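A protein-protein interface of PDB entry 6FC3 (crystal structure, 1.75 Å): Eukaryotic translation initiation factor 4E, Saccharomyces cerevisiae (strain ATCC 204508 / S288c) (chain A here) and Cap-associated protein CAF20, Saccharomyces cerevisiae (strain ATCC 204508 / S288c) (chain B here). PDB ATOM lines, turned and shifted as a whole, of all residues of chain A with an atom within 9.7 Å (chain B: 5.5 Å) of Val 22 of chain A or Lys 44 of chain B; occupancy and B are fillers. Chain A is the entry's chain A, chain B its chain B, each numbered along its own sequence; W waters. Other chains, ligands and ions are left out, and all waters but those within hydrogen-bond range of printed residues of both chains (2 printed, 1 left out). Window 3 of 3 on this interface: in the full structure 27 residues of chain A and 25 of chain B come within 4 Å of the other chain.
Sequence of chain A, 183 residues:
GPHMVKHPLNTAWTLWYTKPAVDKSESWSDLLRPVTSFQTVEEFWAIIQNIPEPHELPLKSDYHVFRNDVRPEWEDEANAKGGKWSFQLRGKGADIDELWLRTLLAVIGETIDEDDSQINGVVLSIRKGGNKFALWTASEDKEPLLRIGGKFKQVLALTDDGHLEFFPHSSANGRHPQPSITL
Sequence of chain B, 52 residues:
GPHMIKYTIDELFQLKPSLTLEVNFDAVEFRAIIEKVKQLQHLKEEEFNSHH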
ATOM      1  N   TYR A  17      12.092  -3.590  26.418  1.00  0.00           N
ATOM      2  CA  TYR A  17      10.654  -3.375  26.366  1.00  0.00           C
ATOM      3  C   TYR A  17       9.958  -4.384  27.264  1.00  0.00           C
ATOM      4  O   TYR A  17      10.243  -5.585  27.197  1.00  0.00           O
ATOM      5  CB  TYR A  17      10.123  -3.490  24.943  1.00  0.00           C
ATOM      6  CG  TYR A  17       8.632  -3.289  24.837  1.00  0.00           C
ATOM      7  CD1 TYR A  17       8.049  -2.087  25.194  1.00  0.00           C
ATOM      8  CD2 TYR A  17       7.816  -4.302  24.368  1.00  0.00           C
ATOM      9  CE1 TYR A  17       6.693  -1.898  25.090  1.00  0.00           C
ATOM     10  CE2 TYR A  17       6.444  -4.125  24.253  1.00  0.00           C
ATOM     11  CZ  TYR A  17       5.889  -2.929  24.613  1.00  0.00           C
ATOM     12  OH  TYR A  17       4.536  -2.753  24.522  1.00  0.00           O
ATOM     13  N   LYS A  19       6.411  -5.911  27.626  1.00  0.00           N
ATOM     14  CA  LYS A  19       5.156  -6.029  26.894  1.00  0.00           C
ATOM     15  C   LYS A  19       4.002  -6.228  27.868  1.00  0.00           C
ATOM     16  O   LYS A  19       4.124  -6.991  28.820  1.00  0.00           O
ATOM     17  CB  LYS A  19       5.197  -7.213  25.931  1.00  0.00           C
ATOM     18  CG  LYS A  19       3.954  -7.326  25.029  1.00  0.00           C
ATOM     19  CD  LYS A  19       3.990  -8.619  24.236  1.00  0.00           C
ATOM     20  CE  LYS A  19       3.441  -9.807  25.017  1.00  0.00           C
ATOM     21  NZ  LYS A  19       1.942  -9.744  25.115  1.00  0.00           N
ATOM     22  N   PRO A  20       2.861  -5.590  27.644  1.00  0.00           N
ATOM     23  CA  PRO A  20       1.704  -5.894  28.476  1.00  0.00           C
ATOM     24  C   PRO A  20       1.273  -7.332  28.277  1.00  0.00           C
ATOM     25  O   PRO A  20       1.253  -7.836  27.156  1.00  0.00           O
ATOM     26  CB  PRO A  20       0.640  -4.932  27.960  1.00  0.00           C
ATOM     27  CG  PRO A  20       1.402  -3.829  27.373  1.00  0.00           C
ATOM     28  CD  PRO A  20       2.583  -4.460  26.747  1.00  0.00           C
ATOM     29  N   ALA A  21       0.887  -7.975  29.366  1.00  0.00           N
ATOM     30  CA  ALA A  21       0.242  -9.275  29.262  1.00  0.00           C
ATOM     31  C   ALA A  21      -1.149  -9.109  28.660  1.00  0.00           C
ATOM     32  O   ALA A  21      -1.934  -8.290  29.133  1.00  0.00           O
ATOM     33  CB  ALA A  21       0.144  -9.920  30.641  1.00  0.00           C
ATOM     34  N   VAL A  22      -1.464  -9.895  27.634  1.00  0.00           N
ATOM     35  CA  VAL A  22      -2.821  -9.901  27.082  1.00  0.00           C
ATOM     36  C   VAL A  22      -3.668 -11.044  27.609  1.00  0.00           C
ATOM     37  O   VAL A  22      -4.894 -11.011  27.445  1.00  0.00           O
ATOM     38  CB  VAL A  22      -2.811  -9.924  25.542  1.00  0.00           C
ATOM     39  CG1 VAL A  22      -2.131  -8.659  25.037  1.00  0.00           C
ATOM     40  CG2 VAL A  22      -2.134 -11.155  25.002  1.00  0.00           C
ATOM     41  N   ASP A  23      -3.047 -12.056  28.218  1.00  0.00           N
ATOM     42  CA  ASP A  23      -3.701 -13.160  28.904  1.00  0.00           C
ATOM     43  C   ASP A  23      -3.196 -13.215  30.337  1.00  0.00           C
ATOM     44  O   ASP A  23      -2.072 -12.789  30.618  1.00  0.00           O
ATOM     45  CB  ASP A  23      -3.392 -14.496  28.227  1.00  0.00           C
ATOM     46  CG  ASP A  23      -4.087 -14.645  26.916  1.00  0.00           C
ATOM     47  OD1 ASP A  23      -4.716 -13.641  26.505  1.00  0.00           O
ATOM     48  OD2 ASP A  23      -4.026 -15.753  26.322  1.00  0.00           O
ATOM     49  N   LYS A  24      -4.009 -13.774  31.240  1.00  0.00           N
ATOM     50  CA  LYS A  24      -3.547 -13.936  32.615  1.00  0.00           C
ATOM     51  C   LYS A  24      -2.270 -14.762  32.668  1.00  0.00           C
ATOM     52  O   LYS A  24      -1.330 -14.442  33.414  1.00  0.00           O
ATOM     53  CB  LYS A  24      -4.637 -14.602  33.464  1.00  0.00           C
ATOM     54  CG  LYS A  24      -5.929 -13.808  33.575  1.00  0.00           C
ATOM     55  CD  LYS A  24      -5.721 -12.517  34.343  1.00  0.00           C
ATOM     56  CE  LYS A  24      -6.992 -11.684  34.393  1.00  0.00           C
ATOM     57  NZ  LYS A  24      -6.679 -10.220  34.418  1.00  0.00           N
ATOM     58  N   SER A  25      -2.212 -15.823  31.873  1.00  0.00           N
ATOM     59  CA  SER A  25      -1.073 -16.717  31.914  1.00  0.00           C
ATOM     60  C   SER A  25       0.219 -16.056  31.460  1.00  0.00           C
ATOM     61  O   SER A  25       1.303 -16.533  31.815  1.00  0.00           O
ATOM     62  CB  SER A  25      -1.359 -17.929  31.040  1.00  0.00           C
ATOM     63  OG  SER A  25      -1.367 -17.554  29.685  1.00  0.00           O
ATOM     64  N   GLU A  26       0.142 -14.993  30.667  1.00  0.00           N
ATOM     65  CA  GLU A  26       1.369 -14.358  30.205  1.00  0.00           C
ATOM     66  C   GLU A  26       2.153 -13.753  31.347  1.00  0.00           C
ATOM     67  O   GLU A  26       3.362 -13.542  31.208  1.00  0.00           O
ATOM     68  CB  GLU A  26       1.055 -13.292  29.159  1.00  0.00           C
ATOM     69  CG  GLU A  26       1.352 -13.759  27.766  1.00  0.00           C
ATOM     70  CD  GLU A  26       1.542 -12.609  26.804  1.00  0.00           C
ATOM     71  OE1 GLU A  26       0.742 -11.650  26.853  1.00  0.00           O
ATOM     72  OE2 GLU A  26       2.503 -12.668  26.014  1.00  0.00           O
ATOM     73  N   SER A  27       1.499 -13.490  32.478  1.00  0.00           N
ATOM     74  CA  SER A  27       2.174 -13.002  33.669  1.00  0.00           C
ATOM     75  C   SER A  27       3.136 -14.026  34.242  1.00  0.00           C
ATOM     76  O   SER A  27       3.951 -13.674  35.103  1.00  0.00           O
ATOM     77  CB  SER A  27       1.145 -12.617  34.726  1.00  0.00           C
ATOM     78  OG  SER A  27       0.323 -11.557  34.262  1.00  0.00           O
ATOM     79  N   TRP A  28       3.061 -15.272  33.790  1.00  0.00           N
ATOM     80  CA  TRP A  28       4.013 -16.299  34.203  1.00  0.00           C
ATOM     81  C   TRP A  28       5.241 -16.355  33.308  1.00  0.00           C
ATOM     82  O   TRP A  28       6.156 -17.136  33.585  1.00  0.00           O
ATOM     83  CB  TRP A  28       3.360 -17.675  34.198  1.00  0.00           C
ATOM     84  CG  TRP A  28       2.144 -17.770  35.026  1.00  0.00           C
ATOM     85  CD1 TRP A  28       1.876 -17.077  36.166  1.00  0.00           C
ATOM     86  CD2 TRP A  28       1.010 -18.602  34.783  1.00  0.00           C
ATOM     87  NE1 TRP A  28       0.650 -17.430  36.653  1.00  0.00           N
ATOM     88  CE2 TRP A  28       0.095 -18.365  35.825  1.00  0.00           C
ATOM     89  CE3 TRP A  28       0.682 -19.527  33.788  1.00  0.00           C
ATOM     90  CZ2 TRP A  28      -1.126 -18.996  35.897  1.00  0.00           C
ATOM     91  CZ3 TRP A  28      -0.532 -20.174  33.875  1.00  0.00           C
ATOM     92  CH2 TRP A  28      -1.424 -19.901  34.922  1.00  0.00           C
ATOM     93  N   SER A  29       5.264 -15.586  32.233  1.00  0.00           N
ATOM     94  CA  SER A  29       6.396 -15.556  31.324  1.00  0.00           C
ATOM     95  C   SER A  29       7.198 -14.273  31.535  1.00  0.00           C
ATOM     96  O   SER A  29       6.769 -13.329  32.210  1.00  0.00           O
ATOM     97  CB  SER A  29       5.915 -15.671  29.870  1.00  0.00           C
ATOM     98  OG  SER A  29       5.153 -14.534  29.498  1.00  0.00           O
ATOM     99  N   LEU A  31       8.153 -11.101  30.254  1.00  0.00           N
ATOM    100  CA  LEU A  31       7.686 -10.112  29.293  1.00  0.00           C
ATOM    101  C   LEU A  31       8.683  -8.974  29.104  1.00  0.00           C
ATOM    102  O   LEU A  31       8.492  -8.129  28.223  1.00  0.00           O
ATOM    103  CB  LEU A  31       6.326  -9.570  29.741  1.00  0.00           C
ATOM    104  CG  LEU A  31       5.258 -10.676  29.899  1.00  0.00           C
ATOM    105  CD1 LEU A  31       3.959 -10.098  30.453  1.00  0.00           C
ATOM    106  CD2 LEU A  31       4.999 -11.389  28.595  1.00  0.00           C
ATOM    107  N   PRO A  58       0.857   0.738  24.327  1.00  0.00           N
ATOM    108  CA  PRO A  58      -0.278   0.225  25.086  1.00  0.00           C
ATOM    109  C   PRO A  58      -0.057   0.365  26.578  1.00  0.00           C
ATOM    110  O   PRO A  58       1.069   0.439  27.074  1.00  0.00           O
ATOM    111  CB  PRO A  58      -0.367  -1.251  24.660  1.00  0.00           C
ATOM    112  CG  PRO A  58       0.970  -1.597  24.103  1.00  0.00           C
ATOM    113  CD  PRO A  58       1.545  -0.308  23.552  1.00  0.00           C
ATOM    114  N   LEU A  59      -1.169   0.372  27.295  1.00  0.00           N
ATOM    115  CA  LEU A  59      -1.121   0.459  28.744  1.00  0.00           C
ATOM    116  C   LEU A  59      -0.355  -0.723  29.323  1.00  0.00           C
ATOM    117  O   LEU A  59      -0.480  -1.858  28.859  1.00  0.00           O
ATOM    118  CB  LEU A  59      -2.527   0.496  29.326  1.00  0.00           C
ATOM    119  CG  LEU A  59      -3.402   1.667  28.941  1.00  0.00           C
ATOM    120  CD1 LEU A  59      -4.739   1.543  29.617  1.00  0.00           C
ATOM    121  CD2 LEU A  59      -2.732   2.973  29.357  1.00  0.00           C
ATOM    122  N   LYS A  60       0.431  -0.439  30.355  1.00  0.00           N
ATOM    123  CA  LYS A  60       1.290  -1.373  31.059  1.00  0.00           C
ATOM    124  C   LYS A  60       2.599  -1.618  30.314  1.00  0.00           C
ATOM    125  O   LYS A  60       3.436  -2.396  30.801  1.00  0.00           O
ATOM    126  CB  LYS A  60       0.564  -2.690  31.375  1.00  0.00           C
ATOM    127  CG  LYS A  60      -0.592  -2.492  32.331  1.00  0.00           C
ATOM    128  CD  LYS A  60      -1.303  -3.793  32.669  1.00  0.00           C
ATOM    129  CE  LYS A  60      -2.676  -3.575  33.293  1.00  0.00           C
ATOM    130  NZ  LYS A  60      -3.396  -4.869  33.568  1.00  0.00           N
ATOM    131  N   SER A  61       2.867  -0.894  29.226  1.00  0.00           N
ATOM    132  CA  SER A  61       4.166  -0.950  28.574  1.00  0.00           C
ATOM    133  C   SER A  61       5.226  -0.270  29.434  1.00  0.00           C
ATOM    134  O   SER A  61       4.942   0.721  30.106  1.00  0.00           O
ATOM    135  CB  SER A  61       4.157  -0.193  27.247  1.00  0.00           C
ATOM    136  OG  SER A  61       3.331  -0.788  26.303  1.00  0.00           O
ATOM    137  N   LYS A 128      -2.660   3.508  33.208  1.00  0.00           N
ATOM    138  CA  LYS A 128      -3.973   4.137  33.252  1.00  0.00           C
ATOM    139  C   LYS A 128      -3.990   5.201  34.338  1.00  0.00           C
ATOM    140  O   LYS A 128      -3.491   4.990  35.448  1.00  0.00           O
ATOM    141  CB  LYS A 128      -5.049   3.080  33.506  1.00  0.00           C
ATOM    142  CG  LYS A 128      -6.432   3.533  33.154  1.00  0.00           C
ATOM    143  CD  LYS A 128      -7.465   2.404  33.288  1.00  0.00           C
ATOM    144  CE  LYS A 128      -8.883   2.974  33.451  1.00  0.00           C
ATOM    145  NZ  LYS A 128      -9.970   1.949  33.366  1.00  0.00           N
ATOM    146  N   VAL B  37      -0.947  -5.864  20.555  1.00  0.00           N
ATOM    147  CA  VAL B  37      -1.377  -5.651  21.937  1.00  0.00           C
ATOM    148  C   VAL B  37      -2.471  -4.584  22.002  1.00  0.00           C
ATOM    149  O   VAL B  37      -3.464  -4.727  22.724  1.00  0.00           O
ATOM    150  CB  VAL B  37      -0.166  -5.298  22.832  1.00  0.00           C
ATOM    151  CG1 VAL B  37      -0.617  -4.809  24.182  1.00  0.00           C
ATOM    152  CG2 VAL B  37       0.733  -6.550  23.031  1.00  0.00           C
ATOM    153  N   GLN B  39      -4.574  -3.704  19.704  1.00  0.00           N
ATOM    154  CA  GLN B  39      -5.797  -4.270  19.140  1.00  0.00           C
ATOM    155  C   GLN B  39      -6.550  -5.068  20.194  1.00  0.00           C
ATOM    156  O   GLN B  39      -7.763  -4.903  20.376  1.00  0.00           O
ATOM    157  CB  GLN B  39      -5.434  -5.156  17.949  1.00  0.00           C
ATOM    158  CG  GLN B  39      -6.573  -5.932  17.358  1.00  0.00           C
ATOM    159  CD  GLN B  39      -6.066  -7.082  16.497  1.00  0.00           C
ATOM    160  OE1 GLN B  39      -5.987  -8.216  16.953  1.00  0.00           O
ATOM    161  NE2 GLN B  39      -5.691  -6.782  15.257  1.00  0.00           N
ATOM    162  N   LEU B  40      -5.837  -5.959  20.898  1.00  0.00           N
ATOM    163  CA  LEU B  40      -6.475  -6.795  21.903  1.00  0.00           C
ATOM    164  C   LEU B  40      -6.970  -5.979  23.091  1.00  0.00           C
ATOM    165  O   LEU B  40      -8.006  -6.309  23.670  1.00  0.00           O
ATOM    166  CB  LEU B  40      -5.503  -7.877  22.366  1.00  0.00           C
ATOM    167  CG  LEU B  40      -5.011  -8.798  21.259  1.00  0.00           C
ATOM    168  CD1 LEU B  40      -3.861  -9.693  21.715  1.00  0.00           C
ATOM    169  CD2 LEU B  40      -6.150  -9.661  20.764  1.00  0.00           C
ATOM    170  N   GLN B  41      -6.219  -4.953  23.516  1.00  0.00           N
ATOM    171  CA  GLN B  41      -6.679  -4.114  24.621  1.00  0.00           C
ATOM    172  C   GLN B  41      -7.950  -3.388  24.245  1.00  0.00           C
ATOM    173  O   GLN B  41      -8.878  -3.257  25.056  1.00  0.00           O
ATOM    174  CB  GLN B  41      -5.605  -3.084  25.015  1.00  0.00           C
ATOM    175  CG  GLN B  41      -4.420  -3.740  25.753  1.00  0.00           C
ATOM    176  CD  GLN B  41      -3.435  -2.727  26.346  1.00  0.00           C
ATOM    177  OE1 GLN B  41      -3.466  -1.516  26.039  1.00  0.00           O
ATOM    178  NE2 GLN B  41      -2.579  -3.215  27.219  1.00  0.00           N
ATOM    179  N   HIS B  42      -7.999  -2.895  23.018  1.00  0.00           N
ATOM    180  CA  HIS B  42      -9.190  -2.185  22.563  1.00  0.00           C
ATOM    181  C   HIS B  42     -10.397  -3.114  22.524  1.00  0.00           C
ATOM    182  O   HIS B  42     -11.500  -2.738  22.944  1.00  0.00           O
ATOM    183  CB  HIS B  42      -8.939  -1.585  21.198  1.00  0.00           C
ATOM    184  CG  HIS B  42     -10.176  -1.037  20.561  1.00  0.00           C
ATOM    185  ND1 HIS B  42     -10.571  -1.378  19.284  1.00  0.00           N
ATOM    186  CD2 HIS B  42     -11.147  -0.235  21.055  1.00  0.00           C
ATOM    187  CE1 HIS B  42     -11.709  -0.760  19.008  1.00  0.00           C
ATOM    188  NE2 HIS B  42     -12.082  -0.078  20.071  1.00  0.00           N
ATOM    189  N   LEU B  43     -10.219  -4.330  22.024  1.00  0.00           N
ATOM    190  CA  LEU B  43     -11.351  -5.245  21.991  1.00  0.00           C
ATOM    191  C   LEU B  43     -11.822  -5.595  23.397  1.00  0.00           C
ATOM    192  O   LEU B  43     -13.026  -5.747  23.628  1.00  0.00           O
ATOM    193  CB  LEU B  43     -10.980  -6.497  21.199  1.00  0.00           C
ATOM    194  CG  LEU B  43     -10.704  -6.205  19.714  1.00  0.00           C
ATOM    195  CD1 LEU B  43     -10.184  -7.419  18.956  1.00  0.00           C
ATOM    196  CD2 LEU B  43     -11.948  -5.687  19.027  1.00  0.00           C
ATOM    197  N   LYS B  44     -10.908  -5.669  24.360  1.00  0.00           N
ATOM    198  CA  LYS B  44     -11.263  -6.146  25.691  1.00  0.00           C
ATOM    199  C   LYS B  44     -11.764  -5.040  26.617  1.00  0.00           C
ATOM    200  O   LYS B  44     -12.541  -5.320  27.536  1.00  0.00           O
ATOM    201  CB  LYS B  44     -10.062  -6.863  26.321  1.00  0.00           C
ATOM    202  CG  LYS B  44      -9.622  -8.111  25.545  1.00  0.00           C
ATOM    203  CD  LYS B  44      -8.535  -8.918  26.267  1.00  0.00           C
ATOM    204  CE  LYS B  44      -9.119  -9.721  27.433  1.00  0.00           C
ATOM    205  NZ  LYS B  44      -8.147 -10.690  28.010  1.00  0.00           N
ATOM    206  N   GLU B  45     -11.358  -3.797  26.406  1.00  0.00           N
ATOM    207  CA  GLU B  45     -11.872  -2.692  27.206  1.00  0.00           C
ATOM    208  C   GLU B  45     -13.268  -2.312  26.732  1.00  0.00           C
ATOM    209  O   GLU B  45     -13.497  -2.140  25.532  1.00  0.00           O
ATOM    210  CB  GLU B  45     -10.954  -1.471  27.117  1.00  0.00           C
ATOM    211  CG  GLU B  45      -9.527  -1.664  27.640  1.00  0.00           C
ATOM    212  CD  GLU B  45      -9.429  -2.670  28.770  1.00  0.00           C
ATOM    213  OE1 GLU B  45      -8.800  -3.731  28.565  1.00  0.00           O
ATOM    214  OE2 GLU B  45      -9.984  -2.395  29.857  1.00  0.00           O
ATOM    215  N   GLU B  46     -14.193  -2.164  27.678  1.00  0.00           N
ATOM    216  CA  GLU B  46     -15.589  -1.859  27.370  1.00  0.00           C
ATOM    217  C   GLU B  46     -15.762  -0.344  27.400  1.00  0.00           C
ATOM    218  O   GLU B  46     -15.915   0.258  28.464  1.00  0.00           O
ATOM    219  CB  GLU B  46     -16.522  -2.564  28.353  1.00  0.00           C
ATOM    220  CG  GLU B  46     -16.336  -4.093  28.377  1.00  0.00           C
ATOM    221  CD  GLU B  46     -17.309  -4.821  29.291  1.00  0.00           C
ATOM    222  OE1 GLU B  46     -18.330  -4.223  29.706  1.00  0.00           O
ATOM    223  OE2 GLU B  46     -17.048  -6.008  29.592  1.00  0.00           O
HETATM  224  O   HOH W   1      -3.181  -5.954  27.987  1.00  0.00           O
HETATM  225  O   HOH W   2      -7.498 -12.780  26.939  1.00  0.00           O
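The backbone carbonyl oxygen (O) of Leu 59 of chain A lies within hydrogen-bond range of the side-chain amide nitrogen (NE2) of Gln 41 of chain B (3.0 Å). O of Val 22 of chain A is in hydrogen-bond range of NZ of Lys 44 of chain B (3.3 Å).
The side-chain hydroxyl (OG) of Ser 61 of chain A is in hydrogen-bond range of the backbone carbonyl oxygen (O) of Pro 58 of chain A. The side-chain amino group (NZ) of Lys 19 of chain A is in salt-bridge range of the side-chain carboxylate (OE1) of Glu 26 of chain A, 2.8 Å away. OE1 of Glu 26 of chain A sits at hydrogen-bond distance from N of Val 22 of chain A, at 2.9 Å. The backbone carbonyl oxygen (O) of Leu 31 of chain A lies within hydrogen-bond range of the backbone NH (N) of Lys 19 of chain A.
Lys 19 of chain A touches Val 37 of chain B (CG to CG2, 3.9 Å). Pro 20 of chain A touches Val 37 of chain B (CG to CG1, 3.9 Å). Pro 20 of chain A touches Gln 41 of chain B (CB to NE2, 3.7 Å). Val 22 of chain A touches Leu 40 of chain B. Pro 58 of chain A touches Val 37 of chain B. Pro 58 of chain A touches Gln 41 of chain B.
Val 22 of chain A touches two residues of chain B. Printed residues of chain A within 4 Å of Lys 44 of chain B: Val 22 (3.3 Å). Of chain A, only Lys 19 (3.9 Å), Pro 20 (3.9 Å) and Pro 58 (3.6 Å) come within 4 Å of Val 37 of chain B. No residue of chain A comes within 4 Å of Glu 45 of chain B. Of the printed residues of chain B, Leu 59 of chain A touches Gln 41 (3.0 Å). Of the printed residues of chain B, Pro 20 of chain A touches Val 37 (3.9 Å) and Gln 41 (3.7 Å). Printed residues of chain A within 4 Å of Gln 41 of chain B: Pro 20, Pro 58 and Leu 59. The nearest printed residue of chain A that does not touch Gln 41 of chain B is Lys 60 of chain A (5.2 Å).
Of the 9 printed residues of chain B, 4 touch a printed residue of chain A. Printed residues of chain B that touch a printed residue of chain A: Val 37, Leu 40, Gln 41 and Lys 44. Hydrophobic or aromatic side chains of chain B within 4 Å of the printed part of chain A: Val 37 and Leu 40. Printed residues of chain A that touch a printed residue of chain B: Lys 19, Pro 20, Val 22, Pro 58 and Leu 59. Hydrophobic or aromatic side chains of chain A that line the printed part of chain B: Pro 20, Val 22, Pro 58 and Leu 59. Among the printed residues, 8 pairs touch across the chains. Among the printed residues, no Asp or Glu carboxylate lies within 4 Å of a Lys or Arg side-chain nitrogen of the other chain.
Water W2 lies within hydrogen-bond range of NZ of Lys 44 of chain B (2.4 Å), OD1 of Asp 23 of chain A (2.9 Å) and O of Val 22 of chain A (3.2 Å). Water W1 bridges the backbone carbonyl oxygen of Ala 21 of chain A (2.9 Å) and the side-chain amide nitrogen of Gln 41 of chain B (2.9 Å).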
